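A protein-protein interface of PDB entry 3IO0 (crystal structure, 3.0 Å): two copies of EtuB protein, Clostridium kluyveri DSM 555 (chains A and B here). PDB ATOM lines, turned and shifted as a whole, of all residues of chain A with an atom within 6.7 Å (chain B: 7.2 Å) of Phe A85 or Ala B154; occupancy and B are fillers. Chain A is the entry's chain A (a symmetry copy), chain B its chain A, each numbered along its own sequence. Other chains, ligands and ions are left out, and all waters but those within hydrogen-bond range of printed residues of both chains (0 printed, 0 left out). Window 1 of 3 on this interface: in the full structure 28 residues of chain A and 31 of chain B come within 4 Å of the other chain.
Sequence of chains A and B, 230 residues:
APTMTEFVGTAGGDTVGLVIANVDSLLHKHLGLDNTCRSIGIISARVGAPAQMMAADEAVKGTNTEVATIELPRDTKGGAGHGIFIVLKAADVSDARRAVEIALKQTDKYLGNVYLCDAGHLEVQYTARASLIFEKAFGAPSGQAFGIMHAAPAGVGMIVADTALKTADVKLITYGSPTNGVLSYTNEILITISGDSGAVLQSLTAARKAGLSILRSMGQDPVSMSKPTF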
ATOM      1  N   LEU A  18       7.145  10.002 -10.119  1.00  0.00           N
ATOM      2  CA  LEU A  18       7.253  10.827  -8.930  1.00  0.00           C
ATOM      3  C   LEU A  18       8.100  12.035  -9.236  1.00  0.00           C
ATOM      4  O   LEU A  18       8.917  12.018 -10.161  1.00  0.00           O
ATOM      5  CB  LEU A  18       7.895  10.046  -7.789  1.00  0.00           C
ATOM      6  CG  LEU A  18       7.177   8.781  -7.337  1.00  0.00           C
ATOM      7  CD1 LEU A  18       8.104   7.930  -6.511  1.00  0.00           C
ATOM      8  CD2 LEU A  18       5.939   9.143  -6.555  1.00  0.00           C
ATOM      9  N   LEU A  31      22.889  11.304  -5.609  1.00  0.00           N
ATOM     10  CA  LEU A  31      22.372  11.493  -6.960  1.00  0.00           C
ATOM     11  C   LEU A  31      23.304  12.482  -7.625  1.00  0.00           C
ATOM     12  O   LEU A  31      24.229  12.981  -6.988  1.00  0.00           O
ATOM     13  CB  LEU A  31      20.948  12.021  -6.908  1.00  0.00           C
ATOM     14  CG  LEU A  31      20.042  11.148  -6.042  1.00  0.00           C
ATOM     15  CD1 LEU A  31      18.865  11.940  -5.559  1.00  0.00           C
ATOM     16  CD2 LEU A  31      19.586   9.903  -6.775  1.00  0.00           C
ATOM     17  N   ILE A  42      11.213  10.841 -11.174  1.00  0.00           N
ATOM     18  CA  ILE A  42      11.455   9.416 -10.986  1.00  0.00           C
ATOM     19  C   ILE A  42      10.508   8.559 -11.812  1.00  0.00           C
ATOM     20  O   ILE A  42       9.304   8.800 -11.845  1.00  0.00           O
ATOM     21  CB  ILE A  42      11.323   9.016  -9.496  1.00  0.00           C
ATOM     22  CG1 ILE A  42      12.359   9.756  -8.646  1.00  0.00           C
ATOM     23  CG2 ILE A  42      11.441   7.490  -9.328  1.00  0.00           C
ATOM     24  CD1 ILE A  42      12.016   9.847  -7.181  1.00  0.00           C
ATOM     25  N   ILE A  43      11.069   7.564 -12.490  1.00  0.00           N
ATOM     26  CA  ILE A  43      10.280   6.473 -13.051  1.00  0.00           C
ATOM     27  C   ILE A  43      10.783   5.219 -12.367  1.00  0.00           C
ATOM     28  O   ILE A  43      11.964   4.893 -12.460  1.00  0.00           O
ATOM     29  CB  ILE A  43      10.410   6.353 -14.595  1.00  0.00           C
ATOM     30  CG1 ILE A  43      10.058   7.674 -15.286  1.00  0.00           C
ATOM     31  CG2 ILE A  43       9.511   5.254 -15.120  1.00  0.00           C
ATOM     32  CD1 ILE A  43       8.598   8.082 -15.144  1.00  0.00           C
ATOM     33  N   SER A  44       9.887   4.543 -11.659  1.00  0.00           N
ATOM     34  CA  SER A  44      10.234   3.356 -10.893  1.00  0.00           C
ATOM     35  C   SER A  44       9.207   2.271 -11.182  1.00  0.00           C
ATOM     36  O   SER A  44       8.012   2.556 -11.175  1.00  0.00           O
ATOM     37  CB  SER A  44      10.251   3.691  -9.396  1.00  0.00           C
ATOM     38  OG  SER A  44      10.861   2.656  -8.632  1.00  0.00           O
ATOM     39  N   ALA A  45       9.651   1.041 -11.437  1.00  0.00           N
ATOM     40  CA  ALA A  45       8.719  -0.048 -11.746  1.00  0.00           C
ATOM     41  C   ALA A  45       9.177  -1.415 -11.277  1.00  0.00           C
ATOM     42  O   ALA A  45      10.384  -1.672 -11.137  1.00  0.00           O
ATOM     43  CB  ALA A  45       8.432  -0.100 -13.222  1.00  0.00           C
ATOM     44  N   ARG A  46       8.205  -2.294 -11.056  1.00  0.00           N
ATOM     45  CA  ARG A  46       8.496  -3.646 -10.619  1.00  0.00           C
ATOM     46  C   ARG A  46       8.836  -4.510 -11.814  1.00  0.00           C
ATOM     47  O   ARG A  46       9.718  -5.357 -11.729  1.00  0.00           O
ATOM     48  CB  ARG A  46       7.311  -4.251  -9.863  1.00  0.00           C
ATOM     49  CG  ARG A  46       6.862  -3.460  -8.624  1.00  0.00           C
ATOM     50  CD  ARG A  46       7.897  -3.466  -7.506  1.00  0.00           C
ATOM     51  NE  ARG A  46       8.388  -4.814  -7.204  1.00  0.00           N
ATOM     52  CZ  ARG A  46       7.691  -5.762  -6.589  1.00  0.00           C
ATOM     53  NH1 ARG A  46       6.444  -5.538  -6.196  1.00  0.00           N
ATOM     54  NH2 ARG A  46       8.248  -6.945  -6.373  1.00  0.00           N
ATOM     55  N   GLY A  48      10.035  -4.907 -15.780  1.00  0.00           N
ATOM     56  CA  GLY A  48      10.637  -4.451 -17.034  1.00  0.00           C
ATOM     57  C   GLY A  48      11.645  -3.345 -16.811  1.00  0.00           C
ATOM     58  O   GLY A  48      11.786  -2.843 -15.696  1.00  0.00           O
ATOM     59  N   ALA A  49      12.348  -2.972 -17.881  1.00  0.00           N
ATOM     60  CA  ALA A  49      13.331  -1.893 -17.832  1.00  0.00           C
ATOM     61  C   ALA A  49      13.539  -1.226 -19.190  1.00  0.00           C
ATOM     62  O   ALA A  49      13.494   0.007 -19.266  1.00  0.00           O
ATOM     63  CB  ALA A  49      14.657  -2.378 -17.256  1.00  0.00           C
ATOM     64  N   THR A  69      20.423   9.058 -12.526  1.00  0.00           N
ATOM     65  CA  THR A  69      20.799   7.671 -12.323  1.00  0.00           C
ATOM     66  C   THR A  69      19.850   6.704 -13.018  1.00  0.00           C
ATOM     67  O   THR A  69      18.644   6.934 -13.054  1.00  0.00           O
ATOM     68  CB  THR A  69      20.943   7.342 -10.806  1.00  0.00           C
ATOM     69  OG1 THR A  69      21.504   6.040 -10.649  1.00  0.00           O
ATOM     70  CG2 THR A  69      19.615   7.371 -10.105  1.00  0.00           C
ATOM     71  N   ILE A  70      20.404   5.639 -13.595  1.00  0.00           N
ATOM     72  CA  ILE A  70      19.600   4.537 -14.123  1.00  0.00           C
ATOM     73  C   ILE A  70      20.093   3.241 -13.493  1.00  0.00           C
ATOM     74  O   ILE A  70      21.208   2.821 -13.763  1.00  0.00           O
ATOM     75  CB  ILE A  70      19.730   4.413 -15.649  1.00  0.00           C
ATOM     76  CG1 ILE A  70      19.438   5.747 -16.331  1.00  0.00           C
ATOM     77  CG2 ILE A  70      18.833   3.292 -16.177  1.00  0.00           C
ATOM     78  CD1 ILE A  70      20.041   5.857 -17.713  1.00  0.00           C
ATOM     79  N   GLU A  71      19.266   2.612 -12.661  1.00  0.00           N
ATOM     80  CA  GLU A  71      19.632   1.362 -11.989  1.00  0.00           C
ATOM     81  C   GLU A  71      18.606   0.250 -12.217  1.00  0.00           C
ATOM     82  O   GLU A  71      17.408   0.517 -12.382  1.00  0.00           O
ATOM     83  CB  GLU A  71      19.826   1.599 -10.500  1.00  0.00           C
ATOM     84  CG  GLU A  71      20.669   2.823 -10.194  1.00  0.00           C
ATOM     85  CD  GLU A  71      20.970   3.004  -8.718  1.00  0.00           C
ATOM     86  OE1 GLU A  71      21.071   1.994  -7.987  1.00  0.00           O
ATOM     87  OE2 GLU A  71      21.115   4.167  -8.288  1.00  0.00           O
ATOM     88  N   LEU A  72      19.085  -0.996 -12.221  1.00  0.00           N
ATOM     89  CA  LEU A  72      18.252  -2.169 -12.509  1.00  0.00           C
ATOM     90  C   LEU A  72      18.300  -3.234 -11.408  1.00  0.00           C
ATOM     91  O   LEU A  72      19.233  -4.025 -11.396  1.00  0.00           O
ATOM     92  CB  LEU A  72      18.767  -2.838 -13.783  1.00  0.00           C
ATOM     93  CG  LEU A  72      18.520  -2.385 -15.230  1.00  0.00           C
ATOM     94  CD1 LEU A  72      18.084  -0.946 -15.374  1.00  0.00           C
ATOM     95  CD2 LEU A  72      19.770  -2.637 -16.074  1.00  0.00           C
ATOM     96  N   PRO A  73      17.291  -3.287 -10.499  1.00  0.00           N
ATOM     97  CA  PRO A  73      17.017  -4.586  -9.787  1.00  0.00           C
ATOM     98  C   PRO A  73      16.546  -5.379 -10.991  1.00  0.00           C
ATOM     99  O   PRO A  73      16.546  -4.756 -12.035  1.00  0.00           O
ATOM    100  CB  PRO A  73      15.855  -4.243  -8.862  1.00  0.00           C
ATOM    101  CG  PRO A  73      15.276  -2.908  -9.373  1.00  0.00           C
ATOM    102  CD  PRO A  73      16.349  -2.205 -10.133  1.00  0.00           C
ATOM    103  N   GLY A  83      12.836  -4.815 -13.178  1.00  0.00           N
ATOM    104  CA  GLY A  83      13.639  -3.977 -12.314  1.00  0.00           C
ATOM    105  C   GLY A  83      13.958  -2.645 -12.988  1.00  0.00           C
ATOM    106  O   GLY A  83      14.898  -2.583 -13.788  1.00  0.00           O
ATOM    107  N   ILE A  84      13.227  -1.566 -12.710  1.00  0.00           N
ATOM    108  CA  ILE A  84      13.705  -0.277 -13.255  1.00  0.00           C
ATOM    109  C   ILE A  84      13.629   0.941 -12.323  1.00  0.00           C
ATOM    110  O   ILE A  84      12.607   1.173 -11.673  1.00  0.00           O
ATOM    111  CB  ILE A  84      13.165   0.023 -14.679  1.00  0.00           C
ATOM    112  CG1 ILE A  84      13.812   1.277 -15.261  1.00  0.00           C
ATOM    113  CG2 ILE A  84      11.687   0.171 -14.682  1.00  0.00           C
ATOM    114  CD1 ILE A  84      15.259   1.112 -15.678  1.00  0.00           C
ATOM    115  N   PHE A  85      14.719   1.705 -12.264  1.00  0.00           N
ATOM    116  CA  PHE A  85      14.782   2.904 -11.431  1.00  0.00           C
ATOM    117  C   PHE A  85      15.538   4.024 -12.136  1.00  0.00           C
ATOM    118  O   PHE A  85      16.769   4.003 -12.234  1.00  0.00           O
ATOM    119  CB  PHE A  85      15.410   2.589 -10.081  1.00  0.00           C
ATOM    120  CG  PHE A  85      15.547   3.779  -9.167  1.00  0.00           C
ATOM    121  CD1 PHE A  85      14.422   4.405  -8.636  1.00  0.00           C
ATOM    122  CD2 PHE A  85      16.807   4.248  -8.802  1.00  0.00           C
ATOM    123  CE1 PHE A  85      14.547   5.504  -7.769  1.00  0.00           C
ATOM    124  CE2 PHE A  85      16.943   5.337  -7.950  1.00  0.00           C
ATOM    125  CZ  PHE A  85      15.805   5.966  -7.426  1.00  0.00           C
ATOM    126  N   ILE A  86      14.775   4.998 -12.629  1.00  0.00           N
ATOM    127  CA  ILE A  86      15.306   6.094 -13.428  1.00  0.00           C
ATOM    128  C   ILE A  86      15.064   7.400 -12.697  1.00  0.00           C
ATOM    129  O   ILE A  86      13.932   7.687 -12.290  1.00  0.00           O
ATOM    130  CB  ILE A  86      14.634   6.144 -14.807  1.00  0.00           C
ATOM    131  CG1 ILE A  86      14.985   4.888 -15.602  1.00  0.00           C
ATOM    132  CG2 ILE A  86      15.062   7.378 -15.569  1.00  0.00           C
ATOM    133  CD1 ILE A  86      14.083   4.635 -16.790  1.00  0.00           C
ATOM    134  N   VAL A  87      16.133   8.174 -12.512  1.00  0.00           N
ATOM    135  CA  VAL A  87      16.031   9.497 -11.910  1.00  0.00           C
ATOM    136  C   VAL A  87      16.554  10.537 -12.884  1.00  0.00           C
ATOM    137  O   VAL A  87      17.698  10.465 -13.327  1.00  0.00           O
ATOM    138  CB  VAL A  87      16.760   9.597 -10.539  1.00  0.00           C
ATOM    139  CG1 VAL A  87      16.681  10.997  -9.982  1.00  0.00           C
ATOM    140  CG2 VAL A  87      16.139   8.644  -9.545  1.00  0.00           C
ATOM    141  N   ALA B  80      10.119  -7.809  -3.242  1.00  0.00           N
ATOM    142  CA  ALA B  80      11.093  -6.917  -3.859  1.00  0.00           C
ATOM    143  C   ALA B  80      12.289  -6.573  -2.932  1.00  0.00           C
ATOM    144  O   ALA B  80      13.123  -5.744  -3.301  1.00  0.00           O
ATOM    145  CB  ALA B  80      10.388  -5.631  -4.291  1.00  0.00           C
ATOM    146  N   ALA B 151      11.292   1.450   0.917  1.00  0.00           N
ATOM    147  CA  ALA B 151      10.044   1.087   0.270  1.00  0.00           C
ATOM    148  C   ALA B 151      10.316   0.598  -1.156  1.00  0.00           C
ATOM    149  O   ALA B 151      11.324   0.979  -1.781  1.00  0.00           O
ATOM    150  CB  ALA B 151       9.088   2.251   0.272  1.00  0.00           C
ATOM    151  N   ALA B 152       9.427  -0.268  -1.643  1.00  0.00           N
ATOM    152  CA  ALA B 152       9.488  -0.787  -2.997  1.00  0.00           C
ATOM    153  C   ALA B 152       8.170  -0.453  -3.656  1.00  0.00           C
ATOM    154  O   ALA B 152       7.132  -0.533  -3.010  1.00  0.00           O
ATOM    155  CB  ALA B 152       9.697  -2.282  -2.985  1.00  0.00           C
ATOM    156  N   PRO B 153       8.194  -0.084  -4.946  1.00  0.00           N
ATOM    157  CA  PRO B 153       9.374   0.055  -5.783  1.00  0.00           C
ATOM    158  C   PRO B 153      10.201   1.232  -5.327  1.00  0.00           C
ATOM    159  O   PRO B 153       9.687   2.126  -4.638  1.00  0.00           O
ATOM    160  CB  PRO B 153       8.789   0.323  -7.169  1.00  0.00           C
ATOM    161  CG  PRO B 153       7.477   0.924  -6.908  1.00  0.00           C
ATOM    162  CD  PRO B 153       6.965   0.228  -5.690  1.00  0.00           C
ATOM    163  N   ALA B 154      11.472   1.230  -5.724  1.00  0.00           N
ATOM    164  CA  ALA B 154      12.467   2.170  -5.205  1.00  0.00           C
ATOM    165  C   ALA B 154      11.997   3.629  -5.163  1.00  0.00           C
ATOM    166  O   ALA B 154      12.400   4.383  -4.279  1.00  0.00           O
ATOM    167  CB  ALA B 154      13.763   2.044  -5.985  1.00  0.00           C
ATOM    168  N   GLY B 155      11.148   4.023  -6.101  1.00  0.00           N
ATOM    169  CA  GLY B 155      10.709   5.406  -6.165  1.00  0.00           C
ATOM    170  C   GLY B 155      10.077   5.884  -4.867  1.00  0.00           C
ATOM    171  O   GLY B 155      10.380   6.981  -4.372  1.00  0.00           O
ATOM    172  N   VAL B 156       9.196   5.047  -4.322  1.00  0.00           N
ATOM    173  CA  VAL B 156       8.542   5.300  -3.049  1.00  0.00           C
ATOM    174  C   VAL B 156       9.601   5.465  -1.968  1.00  0.00           C
ATOM    175  O   VAL B 156       9.510   6.359  -1.129  1.00  0.00           O
ATOM    176  CB  VAL B 156       7.608   4.146  -2.682  1.00  0.00           C
ATOM    177  CG1 VAL B 156       6.688   4.548  -1.538  1.00  0.00           C
ATOM    178  CG2 VAL B 156       6.785   3.725  -3.899  1.00  0.00           C
ATOM    179  N   GLY B 157      10.615   4.608  -2.019  1.00  0.00           N
ATOM    180  CA  GLY B 157      11.778   4.720  -1.157  1.00  0.00           C
ATOM    181  C   GLY B 157      12.406   6.099  -1.133  1.00  0.00           C
ATOM    182  O   GLY B 157      12.780   6.564  -0.061  1.00  0.00           O
ATOM    183  N   MET B 158      12.530   6.751  -2.298  1.00  0.00           N
ATOM    184  CA  MET B 158      13.077   8.127  -2.369  1.00  0.00           C
ATOM    185  C   MET B 158      12.238   9.111  -1.577  1.00  0.00           C
ATOM    186  O   MET B 158      12.767   9.862  -0.759  1.00  0.00           O
ATOM    187  CB  MET B 158      13.167   8.659  -3.801  1.00  0.00           C
ATOM    188  CG  MET B 158      14.555   8.649  -4.447  1.00  0.00           C
ATOM    189  SD  MET B 158      15.958   9.371  -3.568  1.00  0.00           S
ATOM    190  CE  MET B 158      15.185  10.801  -2.857  1.00  0.00           C
ATOM    191  N   ILE B 159      10.932   9.105  -1.836  1.00  0.00           N
ATOM    192  CA  ILE B 159       9.997  10.012  -1.182  1.00  0.00           C
ATOM    193  C   ILE B 159      10.095   9.870   0.337  1.00  0.00           C
ATOM    194  O   ILE B 159      10.214  10.875   1.064  1.00  0.00           O
ATOM    195  CB  ILE B 159       8.562   9.734  -1.649  1.00  0.00           C
ATOM    196  CG1 ILE B 159       8.464   9.806  -3.178  1.00  0.00           C
ATOM    197  CG2 ILE B 159       7.584  10.675  -0.987  1.00  0.00           C
ATOM    198  CD1 ILE B 159       8.639  11.186  -3.778  1.00  0.00           C
ATOM    199  N   VAL B 160      10.058   8.618   0.797  1.00  0.00           N
ATOM    200  CA  VAL B 160      10.286   8.268   2.189  1.00  0.00           C
ATOM    201  C   VAL B 160      11.611   8.877   2.657  1.00  0.00           C
ATOM    202  O   VAL B 160      11.634   9.722   3.558  1.00  0.00           O
ATOM    203  CB  VAL B 160      10.294   6.734   2.360  1.00  0.00           C
ATOM    204  CG1 VAL B 160      10.621   6.326   3.784  1.00  0.00           C
ATOM    205  CG2 VAL B 160       8.974   6.166   1.960  1.00  0.00           C
ATOM    206  N   TYR B 175      23.002   5.432   2.562  1.00  0.00           N
ATOM    207  CA  TYR B 175      22.120   5.556   1.400  1.00  0.00           C
ATOM    208  C   TYR B 175      22.278   4.327   0.521  1.00  0.00           C
ATOM    209  O   TYR B 175      23.376   4.029   0.064  1.00  0.00           O
ATOM    210  CB  TYR B 175      22.393   6.834   0.605  1.00  0.00           C
ATOM    211  CG  TYR B 175      21.699   6.866  -0.736  1.00  0.00           C
ATOM    212  CD1 TYR B 175      20.411   7.386  -0.873  1.00  0.00           C
ATOM    213  CD2 TYR B 175      22.325   6.368  -1.868  1.00  0.00           C
ATOM    214  CE1 TYR B 175      19.763   7.416  -2.109  1.00  0.00           C
ATOM    215  CE2 TYR B 175      21.695   6.386  -3.102  1.00  0.00           C
ATOM    216  CZ  TYR B 175      20.415   6.916  -3.224  1.00  0.00           C
ATOM    217  OH  TYR B 175      19.809   6.920  -4.469  1.00  0.00           O
ATOM    218  N   GLY B 176      21.191   3.609   0.292  1.00  0.00           N
ATOM    219  CA  GLY B 176      21.256   2.382  -0.484  1.00  0.00           C
ATOM    220  C   GLY B 176      20.234   2.412  -1.590  1.00  0.00           C
ATOM    221  O   GLY B 176      19.060   2.691  -1.347  1.00  0.00           O
ATOM    222  N   SER B 177      20.689   2.137  -2.809  1.00  0.00           N
ATOM    223  CA  SER B 177      19.829   2.091  -3.984  1.00  0.00           C
ATOM    224  C   SER B 177      19.941   0.692  -4.598  1.00  0.00           C
ATOM    225  O   SER B 177      20.757  -0.116  -4.133  1.00  0.00           O
ATOM    226  CB  SER B 177      20.284   3.150  -4.971  1.00  0.00           C
ATOM    227  OG  SER B 177      21.570   2.831  -5.451  1.00  0.00           O
ATOM    228  N   PRO B 178      19.141   0.391  -5.644  1.00  0.00           N
ATOM    229  CA  PRO B 178      19.113  -0.980  -6.167  1.00  0.00           C
ATOM    230  C   PRO B 178      20.457  -1.541  -6.593  1.00  0.00           C
ATOM    231  O   PRO B 178      20.628  -2.752  -6.613  1.00  0.00           O
ATOM    232  CB  PRO B 178      18.213  -0.865  -7.392  1.00  0.00           C
ATOM    233  CG  PRO B 178      17.315   0.247  -7.066  1.00  0.00           C
ATOM    234  CD  PRO B 178      18.212   1.252  -6.393  1.00  0.00           C
ATOM    235  N   THR B 179      21.413  -0.678  -6.891  1.00  0.00           N
ATOM    236  CA  THR B 179      22.591  -1.104  -7.615  1.00  0.00           C
ATOM    237  C   THR B 179      23.884  -0.391  -7.199  1.00  0.00           C
ATOM    238  O   THR B 179      24.955  -0.714  -7.703  1.00  0.00           O
ATOM    239  CB  THR B 179      22.272  -1.031  -9.126  1.00  0.00           C
ATOM    240  OG1 THR B 179      21.921  -2.342  -9.570  1.00  0.00           O
ATOM    241  CG2 THR B 179      23.408  -0.412 -10.001  1.00  0.00           C
ATOM    242  N   LEU B 183      22.693  -2.504  -1.519  1.00  0.00           N
ATOM    243  CA  LEU B 183      21.563  -3.433  -1.483  1.00  0.00           C
ATOM    244  C   LEU B 183      21.760  -4.555  -2.486  1.00  0.00           C
ATOM    245  O   LEU B 183      22.394  -4.361  -3.517  1.00  0.00           O
ATOM    246  CB  LEU B 183      20.246  -2.713  -1.797  1.00  0.00           C
ATOM    247  CG  LEU B 183      19.917  -1.344  -1.192  1.00  0.00           C
ATOM    248  CD1 LEU B 183      18.557  -0.929  -1.700  1.00  0.00           C
ATOM    249  CD2 LEU B 183      19.959  -1.334   0.333  1.00  0.00           C
ATOM    250  N   THR B 186      17.680  -5.087  -4.821  1.00  0.00           N
ATOM    251  CA  THR B 186      16.275  -5.053  -4.452  1.00  0.00           C
ATOM    252  C   THR B 186      15.645  -3.847  -5.135  1.00  0.00           C
ATOM    253  O   THR B 186      16.348  -2.934  -5.566  1.00  0.00           O
ATOM    254  CB  THR B 186      16.112  -4.999  -2.921  1.00  0.00           C
ATOM    255  OG1 THR B 186      16.844  -3.891  -2.392  1.00  0.00           O
ATOM    256  CG2 THR B 186      16.659  -6.275  -2.296  1.00  0.00           C
ATOM    257  N   ASN B 187      14.330  -3.836  -5.276  1.00  0.00           N
ATOM    258  CA  ASN B 187      13.703  -2.663  -5.867  1.00  0.00           C
ATOM    259  C   ASN B 187      13.345  -1.643  -4.784  1.00  0.00           C
ATOM    260  O   ASN B 187      12.182  -1.282  -4.616  1.00  0.00           O
ATOM    261  CB  ASN B 187      12.494  -3.047  -6.715  1.00  0.00           C
ATOM    262  CG  ASN B 187      12.162  -2.001  -7.762  1.00  0.00           C
ATOM    263  OD1 ASN B 187      12.356  -0.799  -7.551  1.00  0.00           O
ATOM    264  ND2 ASN B 187      11.649  -2.450  -8.899  1.00  0.00           N
ATOM    265  N   GLU B 188      14.362  -1.182  -4.061  1.00  0.00           N
ATOM    266  CA  GLU B 188      14.163  -0.293  -2.924  1.00  0.00           C
ATOM    267  C   GLU B 188      15.132   0.873  -2.932  1.00  0.00           C
ATOM    268  O   GLU B 188      16.233   0.776  -3.484  1.00  0.00           O
ATOM    269  CB  GLU B 188      14.392  -1.049  -1.617  1.00  0.00           C
ATOM    270  CG  GLU B 188      13.528  -2.269  -1.372  1.00  0.00           C
ATOM    271  CD  GLU B 188      14.133  -3.178  -0.317  1.00  0.00           C
ATOM    272  OE1 GLU B 188      15.377  -3.314  -0.294  1.00  0.00           O
ATOM    273  OE2 GLU B 188      13.377  -3.757   0.493  1.00  0.00           O
ATOM    274  N   ILE B 189      14.716   1.976  -2.310  1.00  0.00           N
ATOM    275  CA  ILE B 189      15.662   2.962  -1.773  1.00  0.00           C
ATOM    276  C   ILE B 189      15.675   2.806  -0.253  1.00  0.00           C
ATOM    277  O   ILE B 189      14.627   2.859   0.388  1.00  0.00           O
ATOM    278  CB  ILE B 189      15.318   4.419  -2.177  1.00  0.00           C
ATOM    279  CG1 ILE B 189      15.601   4.646  -3.663  1.00  0.00           C
ATOM    280  CG2 ILE B 189      16.085   5.422  -1.323  1.00  0.00           C
ATOM    281  CD1 ILE B 189      17.066   4.712  -4.015  1.00  0.00           C
ATOM    282  N   LEU B 190      16.862   2.580   0.308  1.00  0.00           N
ATOM    283  CA  LEU B 190      17.029   2.450   1.755  1.00  0.00           C
ATOM    284  C   LEU B 190      17.816   3.613   2.338  1.00  0.00           C
ATOM    285  O   LEU B 190      18.779   4.088   1.740  1.00  0.00           O
ATOM    286  CB  LEU B 190      17.705   1.128   2.115  1.00  0.00           C
ATOM    287  CG  LEU B 190      17.990   0.847   3.595  1.00  0.00           C
ATOM    288  CD1 LEU B 190      17.539  -0.559   3.995  1.00  0.00           C
ATOM    289  CD2 LEU B 190      19.448   1.073   3.918  1.00  0.00           C
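Of chain B, only Ala B154 and Ile B189 come within 4 Å of Phe A85.
Of the printed residues of chain A, Ala B154 touches Ser A44 (3.3 Å) and Phe A85 (3.6 Å).
Of the printed residues of chain B, Leu A72 touches Thr B179.
Printed residues of chain A within 4 Å of Ala B80: Arg A46.
Gly B176 touches none of the printed residues of chain A.
Leu B190 touches none of the printed residues of chain A.
N of Glu A71 sits at hydrogen-bond distance from O of Phe A85 (2.9 Å).
N of Gly A83 lies within hydrogen-bond range of O of Arg A46 (3.5 Å).
The backbone carbonyl oxygen of Asn B187 lies within hydrogen-bond range of the backbone NH of Ala B154, 2.8 Å away.
N of Ile A42 sits at hydrogen-bond distance from O of Leu A18, at 2.8 Å.
The side-chain carboxylate (OE1) of Glu B188 is in hydrogen-bond range of the side-chain hydroxyl (OG1) of Thr B186.
The backbone carbonyl oxygen (O) of Ile A84 sits at hydrogen-bond distance from the backbone NH (N) of Ala A45 (3.0 Å).
Among the printed residues, pairs that only touch across the chains: Leu A18 with Gly B155, Leu A18 with Val B156, Leu A18 with Ile B159, Leu A31 with Tyr B175, Ile A42 with Gly B155, Ile A42 with Met B158, Ser A44 with Pro B153, Ser A44 with Asn B187, Arg A46 with Ala B80, Arg A46 with Pro B153, Arg A46 with Asn B187, Leu A72 with Thr B179, Pro A73 with Pro B178, Pro A73 with Thr B186, Pro A73 with Asn B187, Phe A85 with Ala B154 and Phe A85 with Ile B189.
No position is printed for both chains.
Printed residues of chain A that touch a printed residue of chain B: Leu A18, Leu A31, Ile A42, Ser A44, Ala A45, Arg A46, Glu A71, Leu A72, Pro A73 and Phe A85.
Among the printed residues, no Asp or Glu carboxylate lies within 4 Å of a Lys or Arg side-chain nitrogen of the other chain.
The side-chain hydroxyl (OG) of Ser A44 sits at hydrogen-bond distance from the backbone NH (N) of Ala B154, 3.3 Å away.
The side-chain amide nitrogen (ND2) of Asn B187 is in hydrogen-bond range of the backbone carbonyl oxygen (O) of Ala A45 (2.7 Å).
The backbone NH (N) of Gly B155 sits at hydrogen-bond distance from the side-chain hydroxyl (OG) of Ser A44, at 2.9 Å.
The backbone NH (N) of Thr B179 sits at hydrogen-bond distance from the side-chain carboxylate (OE1) of Glu A71 (2.9 Å).
OE1 of Glu A71 sits at hydrogen-bond distance from OG of Ser B177 (2.7 Å).
OE1 of Glu A71 sits close to N of Pro B178, at 3.4 Å.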
